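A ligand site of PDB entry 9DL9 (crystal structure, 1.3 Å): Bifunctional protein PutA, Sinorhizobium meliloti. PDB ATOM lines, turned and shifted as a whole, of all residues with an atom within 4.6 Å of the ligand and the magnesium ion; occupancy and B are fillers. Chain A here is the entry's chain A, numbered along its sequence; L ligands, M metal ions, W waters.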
ATOM      1  N   ILE A 705       4.824  -2.853  -7.920  1.00  0.00           N
ATOM      2  CA  ILE A 705       5.093  -4.049  -7.147  1.00  0.00           C
ATOM      3  C   ILE A 705       6.392  -4.644  -7.682  1.00  0.00           C
ATOM      4  O   ILE A 705       6.540  -4.866  -8.891  1.00  0.00           O
ATOM      5  CB  ILE A 705       3.926  -5.032  -7.292  1.00  0.00           C
ATOM      6  CG1 ILE A 705       2.661  -4.469  -6.629  1.00  0.00           C
ATOM      7  CG2 ILE A 705       4.283  -6.371  -6.685  1.00  0.00           C
ATOM      8  CD1 ILE A 705       1.418  -5.242  -6.992  1.00  0.00           C
ATOM      9  N   SER A 706       7.331  -4.870  -6.786  1.00  0.00           N
ATOM     10  CA  SER A 706       8.685  -5.188  -7.195  1.00  0.00           C
ATOM     11  C   SER A 706       9.156  -6.473  -6.542  1.00  0.00           C
ATOM     12  O   SER A 706       8.653  -6.870  -5.480  1.00  0.00           O
ATOM     13  CB  SER A 706       9.635  -4.026  -6.845  1.00  0.00           C
ATOM     14  OG  SER A 706       9.525  -3.697  -5.490  1.00  0.00           O
ATOM     15  N   PRO A 707      10.160  -7.113  -7.126  1.00  0.00           N
ATOM     16  CA  PRO A 707      10.657  -8.396  -6.616  1.00  0.00           C
ATOM     17  C   PRO A 707      11.768  -8.176  -5.586  1.00  0.00           C
ATOM     18  O   PRO A 707      12.332  -7.095  -5.460  1.00  0.00           O
ATOM     19  CB  PRO A 707      11.239  -9.032  -7.879  1.00  0.00           C
ATOM     20  CG  PRO A 707      11.816  -7.865  -8.619  1.00  0.00           C
ATOM     21  CD  PRO A 707      10.827  -6.738  -8.382  1.00  0.00           C
ATOM     22  N   TRP A 708      12.089  -9.250  -4.873  1.00  0.00           N
ATOM     23  CA  TRP A 708      13.128  -9.114  -3.856  1.00  0.00           C
ATOM     24  C   TRP A 708      14.534  -9.084  -4.451  1.00  0.00           C
ATOM     25  O   TRP A 708      15.445  -8.521  -3.826  1.00  0.00           O
ATOM     26  CB  TRP A 708      13.034 -10.242  -2.810  1.00  0.00           C
ATOM     27  CG  TRP A 708      13.582 -11.513  -3.350  1.00  0.00           C
ATOM     28  CD1 TRP A 708      12.874 -12.508  -3.948  1.00  0.00           C
ATOM     29  CD2 TRP A 708      14.960 -11.909  -3.408  1.00  0.00           C
ATOM     30  NE1 TRP A 708      13.723 -13.502  -4.369  1.00  0.00           N
ATOM     31  CE2 TRP A 708      15.009 -13.155  -4.047  1.00  0.00           C
ATOM     32  CE3 TRP A 708      16.146 -11.332  -2.951  1.00  0.00           C
ATOM     33  CZ2 TRP A 708      16.202 -13.830  -4.270  1.00  0.00           C
ATOM     34  CZ3 TRP A 708      17.341 -11.995  -3.193  1.00  0.00           C
ATOM     35  CH2 TRP A 708      17.349 -13.243  -3.833  1.00  0.00           C
ATOM     36  N   ASN A 709      14.730  -9.644  -5.636  1.00  0.00           N
ATOM     37  CA  ASN A 709      16.084 -10.029  -6.019  1.00  0.00           C
ATOM     38  C   ASN A 709      16.913  -8.884  -6.566  1.00  0.00           C
ATOM     39  O   ASN A 709      18.144  -8.960  -6.545  1.00  0.00           O
ATOM     40  CB  ASN A 709      16.025 -11.166  -7.027  1.00  0.00           C
ATOM     41  CG  ASN A 709      15.528 -10.721  -8.357  1.00  0.00           C
ATOM     42  OD1 ASN A 709      14.379 -10.316  -8.492  1.00  0.00           O
ATOM     43  ND2 ASN A 709      16.398 -10.753  -9.359  1.00  0.00           N
ATOM     44  N   PHE A 710      16.275  -7.837  -7.092  1.00  0.00           N
ATOM     45  CA  PHE A 710      16.935  -6.590  -7.427  1.00  0.00           C
ATOM     46  C   PHE A 710      16.227  -5.538  -6.583  1.00  0.00           C
ATOM     47  O   PHE A 710      15.427  -4.739  -7.103  1.00  0.00           O
ATOM     48  CB  PHE A 710      16.828  -6.267  -8.918  1.00  0.00           C
ATOM     49  CG  PHE A 710      17.507  -7.279  -9.825  1.00  0.00           C
ATOM     50  CD1 PHE A 710      18.718  -7.831  -9.483  1.00  0.00           C
ATOM     51  CD2 PHE A 710      16.908  -7.668 -11.019  1.00  0.00           C
ATOM     52  CE1 PHE A 710      19.344  -8.756 -10.323  1.00  0.00           C
ATOM     53  CE2 PHE A 710      17.526  -8.580 -11.867  1.00  0.00           C
ATOM     54  CZ  PHE A 710      18.741  -9.129 -11.501  1.00  0.00           C
ATOM     55  N   ILE A 714      15.215  -2.479  -9.522  1.00  0.00           N
ATOM     56  CA  ILE A 714      13.914  -2.595 -10.172  1.00  0.00           C
ATOM     57  C   ILE A 714      12.890  -1.778  -9.397  1.00  0.00           C
ATOM     58  O   ILE A 714      12.026  -1.105  -9.986  1.00  0.00           O
ATOM     59  CB  ILE A 714      13.503  -4.065 -10.314  1.00  0.00           C
ATOM     60  CG1 ILE A 714      14.462  -4.729 -11.310  1.00  0.00           C
ATOM     61  CG2 ILE A 714      12.026  -4.184 -10.740  1.00  0.00           C
ATOM     62  CD1 ILE A 714      13.906  -5.906 -12.018  1.00  0.00           C
ATOM     63  N   LYS A 732       5.078  -0.943  -3.452  1.00  0.00           N
ATOM     64  CA  LYS A 732       4.926  -2.148  -2.636  1.00  0.00           C
ATOM     65  C   LYS A 732       6.148  -3.010  -2.870  1.00  0.00           C
ATOM     66  O   LYS A 732       6.188  -3.801  -3.826  1.00  0.00           O
ATOM     67  CB  LYS A 732       3.639  -2.890  -3.017  1.00  0.00           C
ATOM     68  CG  LYS A 732       2.946  -3.579  -1.853  1.00  0.00           C
ATOM     69  CD  LYS A 732       3.861  -4.612  -1.194  1.00  0.00           C
ATOM     70  CE  LYS A 732       4.031  -5.845  -2.074  1.00  0.00           C
ATOM     71  NZ  LYS A 732       4.973  -6.825  -1.454  1.00  0.00           N
ATOM     72  N   PRO A 733       7.177  -2.914  -2.038  1.00  0.00           N
ATOM     73  CA  PRO A 733       8.379  -3.723  -2.247  1.00  0.00           C
ATOM     74  C   PRO A 733       8.140  -5.143  -1.765  1.00  0.00           C
ATOM     75  O   PRO A 733       7.242  -5.419  -0.969  1.00  0.00           O
ATOM     76  CB  PRO A 733       9.410  -3.039  -1.347  1.00  0.00           C
ATOM     77  CG  PRO A 733       8.575  -2.520  -0.192  1.00  0.00           C
ATOM     78  CD  PRO A 733       7.271  -2.076  -0.824  1.00  0.00           C
ATOM     79  N   ALA A 734       8.972  -6.050  -2.271  1.00  0.00           N
ATOM     80  CA  ALA A 734       8.888  -7.439  -1.868  1.00  0.00           C
ATOM     81  C   ALA A 734       9.022  -7.557  -0.353  1.00  0.00           C
ATOM     82  O   ALA A 734       9.766  -6.804   0.296  1.00  0.00           O
ATOM     83  CB  ALA A 734      10.015  -8.221  -2.524  1.00  0.00           C
ATOM     84  N   GLU A 735       8.302  -8.523   0.224  1.00  0.00           N
ATOM     85  CA  GLU A 735       8.329  -8.676   1.666  1.00  0.00           C
ATOM     86  C   GLU A 735       9.719  -9.032   2.195  1.00  0.00           C
ATOM     87  O   GLU A 735      10.019  -8.751   3.353  1.00  0.00           O
ATOM     88  CB  GLU A 735       7.301  -9.712   2.124  1.00  0.00           C
ATOM     89  CG  GLU A 735       7.419 -11.087   1.467  1.00  0.00           C
ATOM     90  CD  GLU A 735       6.608 -11.203   0.184  1.00  0.00           C
ATOM     91  OE1 GLU A 735       6.366 -10.176  -0.485  1.00  0.00           O
ATOM     92  OE2 GLU A 735       6.217 -12.343  -0.153  1.00  0.00           O
ATOM     93  N   GLU A 736      10.575  -9.621   1.349  1.00  0.00           N
ATOM     94  CA  GLU A 736      11.881 -10.036   1.830  1.00  0.00           C
ATOM     95  C   GLU A 736      12.836  -8.859   1.984  1.00  0.00           C
ATOM     96  O   GLU A 736      13.740  -8.923   2.829  1.00  0.00           O
ATOM     97  CB  GLU A 736      12.495 -11.045   0.858  1.00  0.00           C
ATOM     98  CG  GLU A 736      11.715 -12.346   0.690  1.00  0.00           C
ATOM     99  CD  GLU A 736      10.720 -12.314  -0.461  1.00  0.00           C
ATOM    100  OE1 GLU A 736      10.357 -11.205  -0.919  1.00  0.00           O
ATOM    101  OE2 GLU A 736      10.314 -13.400  -0.920  1.00  0.00           O
ATOM    102  N   GLY A 763       5.013  -4.913   2.931  1.00  0.00           N
ATOM    103  CA  GLY A 763       4.141  -6.028   3.242  1.00  0.00           C
ATOM    104  C   GLY A 763       4.247  -7.089   2.181  1.00  0.00           C
ATOM    105  O   GLY A 763       5.060  -7.004   1.260  1.00  0.00           O
ATOM    106  N   ASP A 764       3.390  -8.100   2.315  1.00  0.00           N
ATOM    107  CA  ASP A 764       3.469  -9.275   1.460  1.00  0.00           C
ATOM    108  C   ASP A 764       2.529  -9.113   0.259  1.00  0.00           C
ATOM    109  O   ASP A 764       2.074  -8.009  -0.061  1.00  0.00           O
ATOM    110  CB  ASP A 764       3.254 -10.553   2.281  1.00  0.00           C
ATOM    111  CG  ASP A 764       1.883 -10.616   2.934  1.00  0.00           C
ATOM    112  OD1 ASP A 764       0.963  -9.923   2.457  1.00  0.00           O
ATOM    113  OD2 ASP A 764       1.717 -11.354   3.927  1.00  0.00           O
ATOM    114  N   GLY A 765       2.237 -10.218  -0.414  1.00  0.00           N
ATOM    115  CA  GLY A 765       1.405 -10.172  -1.605  1.00  0.00           C
ATOM    116  C   GLY A 765       0.015  -9.663  -1.351  1.00  0.00           C
ATOM    117  O   GLY A 765      -0.644  -9.174  -2.277  1.00  0.00           O
ATOM    118  N   GLY A 768       0.134  -6.012  -1.989  1.00  0.00           N
ATOM    119  CA  GLY A 768       0.130  -5.829  -3.432  1.00  0.00           C
ATOM    120  C   GLY A 768      -1.252  -6.024  -4.014  1.00  0.00           C
ATOM    121  O   GLY A 768      -1.717  -5.211  -4.822  1.00  0.00           O
ATOM    122  N   ALA A 769      -1.938  -7.099  -3.612  1.00  0.00           N
ATOM    123  CA  ALA A 769      -3.246  -7.396  -4.181  1.00  0.00           C
ATOM    124  C   ALA A 769      -4.265  -6.333  -3.786  1.00  0.00           C
ATOM    125  O   ALA A 769      -5.104  -5.943  -4.611  1.00  0.00           O
ATOM    126  CB  ALA A 769      -3.713  -8.776  -3.718  1.00  0.00           C
ATOM    127  N   PHE A 782       4.387  -4.363 -12.502  1.00  0.00           N
ATOM    128  CA  PHE A 782       4.731  -5.555 -11.764  1.00  0.00           C
ATOM    129  C   PHE A 782       6.005  -6.156 -12.343  1.00  0.00           C
ATOM    130  O   PHE A 782       6.092  -6.375 -13.563  1.00  0.00           O
ATOM    131  CB  PHE A 782       3.632  -6.605 -11.894  1.00  0.00           C
ATOM    132  CG  PHE A 782       3.981  -7.886 -11.232  1.00  0.00           C
ATOM    133  CD1 PHE A 782       3.878  -8.011  -9.863  1.00  0.00           C
ATOM    134  CD2 PHE A 782       4.477  -8.963 -11.955  1.00  0.00           C
ATOM    135  CE1 PHE A 782       4.227  -9.173  -9.222  1.00  0.00           C
ATOM    136  CE2 PHE A 782       4.820 -10.127 -11.321  1.00  0.00           C
ATOM    137  CZ  PHE A 782       4.686 -10.232  -9.953  1.00  0.00           C
ATOM    138  N   THR A 783       6.951  -6.444 -11.473  1.00  0.00           N
ATOM    139  CA  THR A 783       8.071  -7.304 -11.820  1.00  0.00           C
ATOM    140  C   THR A 783       8.124  -8.398 -10.771  1.00  0.00           C
ATOM    141  O   THR A 783       8.119  -8.108  -9.577  1.00  0.00           O
ATOM    142  CB  THR A 783       9.380  -6.526 -11.900  1.00  0.00           C
ATOM    143  OG1 THR A 783       9.227  -5.472 -12.853  1.00  0.00           O
ATOM    144  CG2 THR A 783      10.510  -7.429 -12.351  1.00  0.00           C
ATOM    145  N   GLY A 784       8.150  -9.645 -11.213  1.00  0.00           N
ATOM    146  CA  GLY A 784       8.038 -10.756 -10.296  1.00  0.00           C
ATOM    147  C   GLY A 784       7.792 -12.024 -11.076  1.00  0.00           C
ATOM    148  O   GLY A 784       8.075 -12.091 -12.277  1.00  0.00           O
ATOM    149  N   SER A 785       7.264 -13.025 -10.386  1.00  0.00           N
ATOM    150  CA  SER A 785       7.077 -14.309 -11.035  1.00  0.00           C
ATOM    151  C   SER A 785       5.877 -14.285 -11.989  1.00  0.00           C
ATOM    152  O   SER A 785       4.918 -13.521 -11.803  1.00  0.00           O
ATOM    153  CB  SER A 785       6.865 -15.398  -9.990  1.00  0.00           C
ATOM    154  OG  SER A 785       5.710 -15.145  -9.226  1.00  0.00           O
ATOM    155  N   VAL A 788       2.509 -15.017 -10.209  1.00  0.00           N
ATOM    156  CA  VAL A 788       1.895 -13.884  -9.520  1.00  0.00           C
ATOM    157  C   VAL A 788       1.347 -12.879 -10.521  1.00  0.00           C
ATOM    158  O   VAL A 788       0.250 -12.333 -10.329  1.00  0.00           O
ATOM    159  CB  VAL A 788       2.889 -13.245  -8.530  1.00  0.00           C
ATOM    160  CG1 VAL A 788       2.345 -11.922  -8.032  1.00  0.00           C
ATOM    161  CG2 VAL A 788       3.130 -14.177  -7.343  1.00  0.00           C
ATOM    162  N   LEU A 791      -2.053 -13.853 -11.466  1.00  0.00           N
ATOM    163  CA  LEU A 791      -3.058 -13.493 -10.484  1.00  0.00           C
ATOM    164  C   LEU A 791      -3.439 -12.022 -10.598  1.00  0.00           C
ATOM    165  O   LEU A 791      -4.627 -11.663 -10.497  1.00  0.00           O
ATOM    166  CB  LEU A 791      -2.532 -13.784  -9.081  1.00  0.00           C
ATOM    167  CG  LEU A 791      -2.285 -15.248  -8.730  1.00  0.00           C
ATOM    168  CD1 LEU A 791      -1.594 -15.370  -7.382  1.00  0.00           C
ATOM    169  CD2 LEU A 791      -3.586 -16.015  -8.732  1.00  0.00           C
ATOM    170  N   ILE A 792      -2.450 -11.162 -10.827  1.00  0.00           N
ATOM    171  CA  ILE A 792      -2.728  -9.735 -11.024  1.00  0.00           C
ATOM    172  C   ILE A 792      -3.526  -9.508 -12.310  1.00  0.00           C
ATOM    173  O   ILE A 792      -4.480  -8.714 -12.323  1.00  0.00           O
ATOM    174  CB  ILE A 792      -1.414  -8.937 -11.012  1.00  0.00           C
ATOM    175  CG1 ILE A 792      -0.832  -8.976  -9.611  1.00  0.00           C
ATOM    176  CG2 ILE A 792      -1.639  -7.494 -11.469  1.00  0.00           C
ATOM    177  CD1 ILE A 792       0.576  -8.435  -9.519  1.00  0.00           C
ATOM    178  N   GLN A 795      -7.056 -10.210 -11.495  1.00  0.00           N
ATOM    179  CA  GLN A 795      -7.656  -9.122 -10.726  1.00  0.00           C
ATOM    180  C   GLN A 795      -8.036  -7.970 -11.636  1.00  0.00           C
ATOM    181  O   GLN A 795      -9.128  -7.398 -11.512  1.00  0.00           O
ATOM    182  CB  GLN A 795      -6.666  -8.586  -9.700  1.00  0.00           C
ATOM    183  CG  GLN A 795      -6.486  -9.357  -8.420  1.00  0.00           C
ATOM    184  CD  GLN A 795      -5.584  -8.602  -7.444  1.00  0.00           C
ATOM    185  OE1 GLN A 795      -4.363  -8.588  -7.602  1.00  0.00           O
ATOM    186  NE2 GLN A 795      -6.183  -7.943  -6.470  1.00  0.00           N
ATOM    187  N   GLU A 812       6.635  -7.869 -15.934  1.00  0.00           N
ATOM    188  CA  GLU A 812       7.953  -8.348 -16.364  1.00  0.00           C
ATOM    189  C   GLU A 812       8.272  -9.533 -15.471  1.00  0.00           C
ATOM    190  O   GLU A 812       8.355  -9.394 -14.254  1.00  0.00           O
ATOM    191  CB  GLU A 812       8.947  -7.212 -16.256  1.00  0.00           C
ATOM    192  CG  GLU A 812       8.562  -6.029 -17.153  1.00  0.00           C
ATOM    193  CD  GLU A 812       8.435  -6.434 -18.626  1.00  0.00           C
ATOM    194  OE1 GLU A 812       9.476  -6.535 -19.300  1.00  0.00           O
ATOM    195  OE2 GLU A 812       7.299  -6.642 -19.112  1.00  0.00           O
ATOM    196  N   THR A 813       8.386 -10.714 -16.072  1.00  0.00           N
ATOM    197  CA  THR A 813       8.259 -11.959 -15.347  1.00  0.00           C
ATOM    198  C   THR A 813       9.500 -12.840 -15.570  1.00  0.00           C
ATOM    199  O   THR A 813      10.595 -12.367 -15.881  1.00  0.00           O
ATOM    200  CB  THR A 813       6.887 -12.586 -15.604  1.00  0.00           C
ATOM    201  OG1 THR A 813       6.667 -12.686 -17.021  1.00  0.00           O
ATOM    202  CG2 THR A 813       5.813 -11.697 -15.006  1.00  0.00           C
ATOM    203  N   GLY A 814       9.346 -14.137 -15.355  1.00  0.00           N
ATOM    204  CA  GLY A 814      10.489 -15.025 -15.245  1.00  0.00           C
ATOM    205  C   GLY A 814      11.093 -15.440 -16.570  1.00  0.00           C
ATOM    206  O   GLY A 814      10.612 -15.088 -17.655  1.00  0.00           O
ATOM    207  N   GLY A 815      12.155 -16.227 -16.482  1.00  0.00           N
ATOM    208  CA  GLY A 815      12.850 -16.697 -17.660  1.00  0.00           C
ATOM    209  C   GLY A 815      13.191 -18.164 -17.506  1.00  0.00           C
ATOM    210  O   GLY A 815      13.182 -18.725 -16.416  1.00  0.00           O
ATOM    211  N   CYS A 846      16.674 -12.744 -12.711  1.00  0.00           N
ATOM    212  CA  CYS A 846      15.720 -13.210 -13.700  1.00  0.00           C
ATOM    213  C   CYS A 846      16.405 -13.597 -14.998  1.00  0.00           C
ATOM    214  O   CYS A 846      15.905 -14.454 -15.733  1.00  0.00           O
ATOM    215  CB  CYS A 846      14.681 -12.129 -13.937  1.00  0.00           C
ATOM    216  SG  CYS A 846      15.347 -10.511 -14.386  1.00  0.00           S
ATOM    217  N   GLU A 942      10.516 -22.072 -14.201  1.00  0.00           N
ATOM    218  CA  GLU A 942      11.736 -21.416 -13.749  1.00  0.00           C
ATOM    219  C   GLU A 942      12.083 -21.876 -12.336  1.00  0.00           C
ATOM    220  O   GLU A 942      11.214 -21.934 -11.464  1.00  0.00           O
ATOM    221  CB  GLU A 942      11.475 -19.910 -13.748  1.00  0.00           C
ATOM    222  CG  GLU A 942      12.605 -19.050 -13.197  1.00  0.00           C
ATOM    223  CD  GLU A 942      12.144 -17.627 -12.976  1.00  0.00           C
ATOM    224  OE1 GLU A 942      11.110 -17.446 -12.293  1.00  0.00           O
ATOM    225  OE2 GLU A 942      12.790 -16.688 -13.473  1.00  0.00           O
ATOM    226  N   PHE A 944      14.420 -20.647  -9.465  1.00  0.00           N
ATOM    227  CA  PHE A 944      15.086 -19.374  -9.218  1.00  0.00           C
ATOM    228  C   PHE A 944      16.155 -19.601  -8.153  1.00  0.00           C
ATOM    229  O   PHE A 944      15.994 -19.263  -6.979  1.00  0.00           O
ATOM    230  CB  PHE A 944      14.056 -18.336  -8.793  1.00  0.00           C
ATOM    231  CG  PHE A 944      14.513 -16.924  -8.978  1.00  0.00           C
ATOM    232  CD1 PHE A 944      14.656 -16.390 -10.242  1.00  0.00           C
ATOM    233  CD2 PHE A 944      14.739 -16.105  -7.881  1.00  0.00           C
ATOM    234  CE1 PHE A 944      15.065 -15.062 -10.406  1.00  0.00           C
ATOM    235  CE2 PHE A 944      15.136 -14.785  -8.046  1.00  0.00           C
ATOM    236  CZ  PHE A 944      15.315 -14.269  -9.302  1.00  0.00           C
ATOM    237  N   LEU A 972      13.217 -14.444 -22.202  1.00  0.00           N
ATOM    238  CA  LEU A 972      13.847 -13.342 -21.483  1.00  0.00           C
ATOM    239  C   LEU A 972      15.259 -13.123 -22.003  1.00  0.00           C
ATOM    240  O   LEU A 972      15.456 -12.349 -22.948  1.00  0.00           O
ATOM    241  CB  LEU A 972      13.758 -13.546 -19.971  1.00  0.00           C
ATOM    242  CG  LEU A 972      14.209 -12.341 -19.131  1.00  0.00           C
ATOM    243  CD1 LEU A 972      13.475 -11.069 -19.555  1.00  0.00           C
ATOM    244  CD2 LEU A 972      13.962 -12.635 -17.656  1.00  0.00           C
ATOM    245  N   PHE A1012      15.911  -3.872 -21.116  1.00  0.00           N
ATOM    246  CA  PHE A1012      15.758  -5.220 -20.606  1.00  0.00           C
ATOM    247  C   PHE A1012      14.297  -5.596 -20.528  1.00  0.00           C
ATOM    248  O   PHE A1012      13.487  -4.847 -19.973  1.00  0.00           O
ATOM    249  CB  PHE A1012      16.386  -5.367 -19.217  1.00  0.00           C
ATOM    250  CG  PHE A1012      16.384  -6.774 -18.750  1.00  0.00           C
ATOM    251  CD1 PHE A1012      17.362  -7.652 -19.195  1.00  0.00           C
ATOM    252  CD2 PHE A1012      15.378  -7.255 -17.909  1.00  0.00           C
ATOM    253  CE1 PHE A1012      17.358  -8.969 -18.799  1.00  0.00           C
ATOM    254  CE2 PHE A1012      15.377  -8.590 -17.498  1.00  0.00           C
ATOM    255  CZ  PHE A1012      16.362  -9.440 -17.940  1.00  0.00           C
ATOM    256  N   SER A1018       7.712 -14.344 -20.225  1.00  0.00           N
ATOM    257  CA  SER A1018       8.705 -13.491 -19.589  1.00  0.00           C
ATOM    258  C   SER A1018       8.318 -12.021 -19.510  1.00  0.00           C
ATOM    259  O   SER A1018       9.017 -11.253 -18.847  1.00  0.00           O
ATOM    260  CB  SER A1018      10.041 -13.597 -20.320  1.00  0.00           C
ATOM    261  OG  SER A1018      10.507 -14.932 -20.274  1.00  0.00           O
HETATM  262  P1  LIG L   1       7.233 -12.737  -6.609  1.00  0.00           P
HETATM  263  O1  LIG L   1       6.306 -13.065  -7.794  1.00  0.00           O
HETATM  264  O2  LIG L   1       7.357 -13.734  -5.550  1.00  0.00           O
HETATM  265  O3  LIG L   1       6.928 -11.477  -5.855  1.00  0.00           O
HETATM  266  C1  LIG L   1       6.980 -10.250  -6.544  1.00  0.00           C
HETATM  267  C2  LIG L   1       6.133  -9.172  -5.880  1.00  0.00           C
HETATM  268  O4  LIG L   1       4.756  -9.451  -6.049  1.00  0.00           O
HETATM  269  C3  LIG L   1       6.383  -8.929  -4.418  1.00  0.00           C
HETATM  270  O5  LIG L   1       6.372  -7.589  -4.081  1.00  0.00           O
HETATM  271  C4  LIG L   1       5.278  -9.672  -3.788  1.00  0.00           C
HETATM  272  O6  LIG L   1       4.985  -9.182  -2.522  1.00  0.00           O
HETATM  273  C5  LIG L   1       4.197  -9.374  -4.753  1.00  0.00           C
HETATM  274  N1  LIG L   1       3.085 -10.280  -4.723  1.00  0.00           N
HETATM  275  C6  LIG L   1       3.050 -11.610  -4.366  1.00  0.00           C
HETATM  276  N2  LIG L   1       1.806 -12.069  -4.524  1.00  0.00           N
HETATM  277  C7  LIG L   1       0.995 -11.064  -4.996  1.00  0.00           C
HETATM  278  C8  LIG L   1      -0.345 -10.964  -5.328  1.00  0.00           C
HETATM  279  N3  LIG L   1      -1.204 -12.114  -5.210  1.00  0.00           N
HETATM  280  N4  LIG L   1      -0.817  -9.807  -5.770  1.00  0.00           N
HETATM  281  C9  LIG L   1      -0.053  -8.691  -5.899  1.00  0.00           C
HETATM  282  N5  LIG L   1       1.261  -8.750  -5.577  1.00  0.00           N
HETATM  283  C10 LIG L   1       1.787  -9.898  -5.133  1.00  0.00           C
HETATM  284  O7  LIG L   1       8.675 -12.586  -7.061  1.00  0.00           O
HETATM  285  P2  LIG L   1      10.091 -12.383  -6.326  1.00  0.00           P
HETATM  286  O8  LIG L   1      10.435 -13.701  -5.725  1.00  0.00           O
HETATM  287  O9  LIG L   1      10.119 -11.215  -5.392  1.00  0.00           O
HETATM  288  O10 LIG L   1      11.094 -12.126  -7.545  1.00  0.00           O
HETATM  289  C11 LIG L   1      11.538 -13.207  -8.329  1.00  0.00           C
HETATM  290  C12 LIG L   1      10.833 -13.336  -9.676  1.00  0.00           C
HETATM  291  O11 LIG L   1      10.837 -12.126 -10.370  1.00  0.00           O
HETATM  292  C13 LIG L   1      11.458 -14.359 -10.555  1.00  0.00           C
HETATM  293  O12 LIG L   1      10.509 -15.137 -11.176  1.00  0.00           O
HETATM  294  C14 LIG L   1      12.189 -13.543 -11.535  1.00  0.00           C
HETATM  295  O13 LIG L   1      12.488 -14.167 -12.741  1.00  0.00           O
HETATM  296  C15 LIG L   1      11.267 -12.380 -11.675  1.00  0.00           C
HETATM  297  N6  LIG L   1      11.975 -11.228 -12.143  1.00  0.00           N
HETATM  298  C16 LIG L   1      11.773 -10.756 -13.463  1.00  0.00           C
HETATM  299  C17 LIG L   1      12.494  -9.644 -13.864  1.00  0.00           C
HETATM  300  C18 LIG L   1      12.358  -9.085 -15.238  1.00  0.00           C
HETATM  301  O14 LIG L   1      12.909  -8.040 -15.511  1.00  0.00           O
HETATM  302  N7  LIG L   1      11.582  -9.790 -16.194  1.00  0.00           N
HETATM  303  C19 LIG L   1      13.383  -9.016 -12.968  1.00  0.00           C
HETATM  304  C20 LIG L   1      13.610  -9.511 -11.670  1.00  0.00           C
HETATM  305  C21 LIG L   1      12.897 -10.622 -11.262  1.00  0.00           C
HETATM  306 MG    MG M   1       7.123 -14.593  -3.672  1.00  0.00          MG
HETATM  307  O   HOH W   1      10.570  -9.099 -19.002  1.00  0.00           O
HETATM  308  O   HOH W   2       7.176 -15.418  -1.834  1.00  0.00           O
HETATM  309  O   HOH W   3       6.517 -12.645  -2.832  1.00  0.00           O
HETATM  310  O   HOH W   4      15.581  -7.027 -14.664  1.00  0.00           O
HETATM  311  O   HOH W   5       7.490 -16.348  -4.561  1.00  0.00           O
HETATM  312  O   HOH W   6       8.738 -11.187  -3.129  1.00  0.00           O
HETATM  313  O   HOH W   7       8.328 -16.814 -13.204  1.00  0.00           O
HETATM  314  O   HOH W   8       5.057 -14.778  -3.916  1.00  0.00           O
HETATM  315  O   HOH W   9      12.571  -5.488 -16.077  1.00  0.00           O
HETATM  316  O   HOH W  10       9.219 -14.219  -3.419  1.00  0.00           O
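O6 of the ligand lies within hydrogen-bond range of NZ of Lys 732.
The backbone NH (N) of Ser 785 sits at hydrogen-bond distance from an oxygen (O1) of the ligand, 2.8 Å away.
The side-chain hydroxyl of Ser 785 lies within hydrogen-bond range of an oxygen (O1) of the ligand (2.6 Å).
An oxygen (O12) of the ligand sits at hydrogen-bond distance from the side-chain carboxylate of Glu 942, at 2.6 Å.
O6 of the ligand lies within hydrogen-bond range of OE1 of Glu 735.
The backbone carbonyl oxygen of Ser 706 sits at hydrogen-bond distance from an oxygen (O5) of the ligand (2.8 Å).
The backbone carbonyl oxygen of Thr 813 sits at hydrogen-bond distance from a nitrogen (N7) of the ligand, at 2.8 Å.
O9 of the ligand lies within hydrogen-bond range of N of Trp 708 (2.8 Å).
The side-chain sulfur (SG) of Cys 846 lies close to an oxygen (O14) of the ligand (3.6 Å).
The side-chain carboxylate (OE1) of Glu 735 is in salt-bridge range of the side-chain amino group (NZ) of Lys 732 (3.8 Å).
The backbone NH (N) of Ser 706 sits at hydrogen-bond distance from the backbone carbonyl oxygen (O) of Lys 732, at 3.3 Å.
The backbone carbonyl oxygen (O) of Asp 764 is in hydrogen-bond range of the side-chain amino group (NZ) of Lys 732, at 3.4 Å.
OG of Ser 785 lies close to N of Val 788.
The backbone NH (N) of Gly 784 lies within hydrogen-bond range of the backbone carbonyl oxygen (O) of Glu 812 (3.1 Å).
N of Thr 783 is in hydrogen-bond range of O of Ile 705, at 3.1 Å.
The side-chain hydroxyl (OG) of Ser 1018 lies within hydrogen-bond range of the backbone carbonyl oxygen (O) of Gly 814 (2.6 Å).
O of Ala 769 is in hydrogen-bond range of NE2 of Gln 795, 2.9 Å away.
The backbone carbonyl oxygen (O) of Gly 784 lies close to an oxygen (O11) of the ligand (3.4 Å).
Residues that only touch the ligand: Ile 705, Pro 707, Asn 709, Phe 710, Ile 714, Pro 733, Ala 734, Asp 764, Gly 765, Gly 768, Ala 769, Phe 782, Thr 783, Val 788, Leu 791, Ile 792, Glu 812, Gly 814, Phe 944, Leu 972, Phe 1012 and Ser 1018.
31 residues have an atom within 4 Å of the ligand: Ile 705, Ser 706, Pro 707, Trp 708, Asn 709, Phe 710, Ile 714, Lys 732, Pro 733, Ala 734, Glu 735, Asp 764, Gly 765, Gly 768, Ala 769, Phe 782, Thr 783, Gly 784, Ser 785, Val 788, Leu 791, Ile 792, Glu 812, Thr 813, Gly 814, Cys 846, Glu 942, Phe 944, Leu 972, Phe 1012 and Ser 1018.
No residue comes within 4 Å of the magnesium ion.
The magnesium ion is bound by water W5.
Water W2 is bound to the magnesium ion, at 2.0 Å.
An oxygen (O2) of the ligand is bound to the magnesium ion, 2.1 Å away.
Water W8 binds the magnesium ion (2.1 Å).
Water W10 is bound to the magnesium ion (2.1 Å).
The magnesium ion is bound by water W3 (2.2 Å).
The magnesium ion has six donor atoms within binding distance.
Water W10 bridges O8 of the ligand (2.7 Å) and OE2 of Glu 736 (2.8 Å).
Water W3 lies within hydrogen-bond range of the side-chain carboxylate (OE2) of Glu 735 (2.7 Å) and an oxygen (O3) of the ligand (3.3 Å).
Water W6 lies within hydrogen-bond range of O9 of the ligand and OE1 of Glu 736.
Water W4 lies within hydrogen-bond range of an oxygen (O14) of the ligand (3.0 Å) and the side-chain sulfur (SG) of Cys 846 (3.5 Å).
Water W1 lies within hydrogen-bond range of O of Ser 1018 (2.7 Å), OE1 of Glu 812 (2.8 Å) and N7 of the ligand (3.1 Å).
Water W7 bridges OE1 of Glu 942 (3.0 Å) and O12 of the ligand (3.4 Å).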
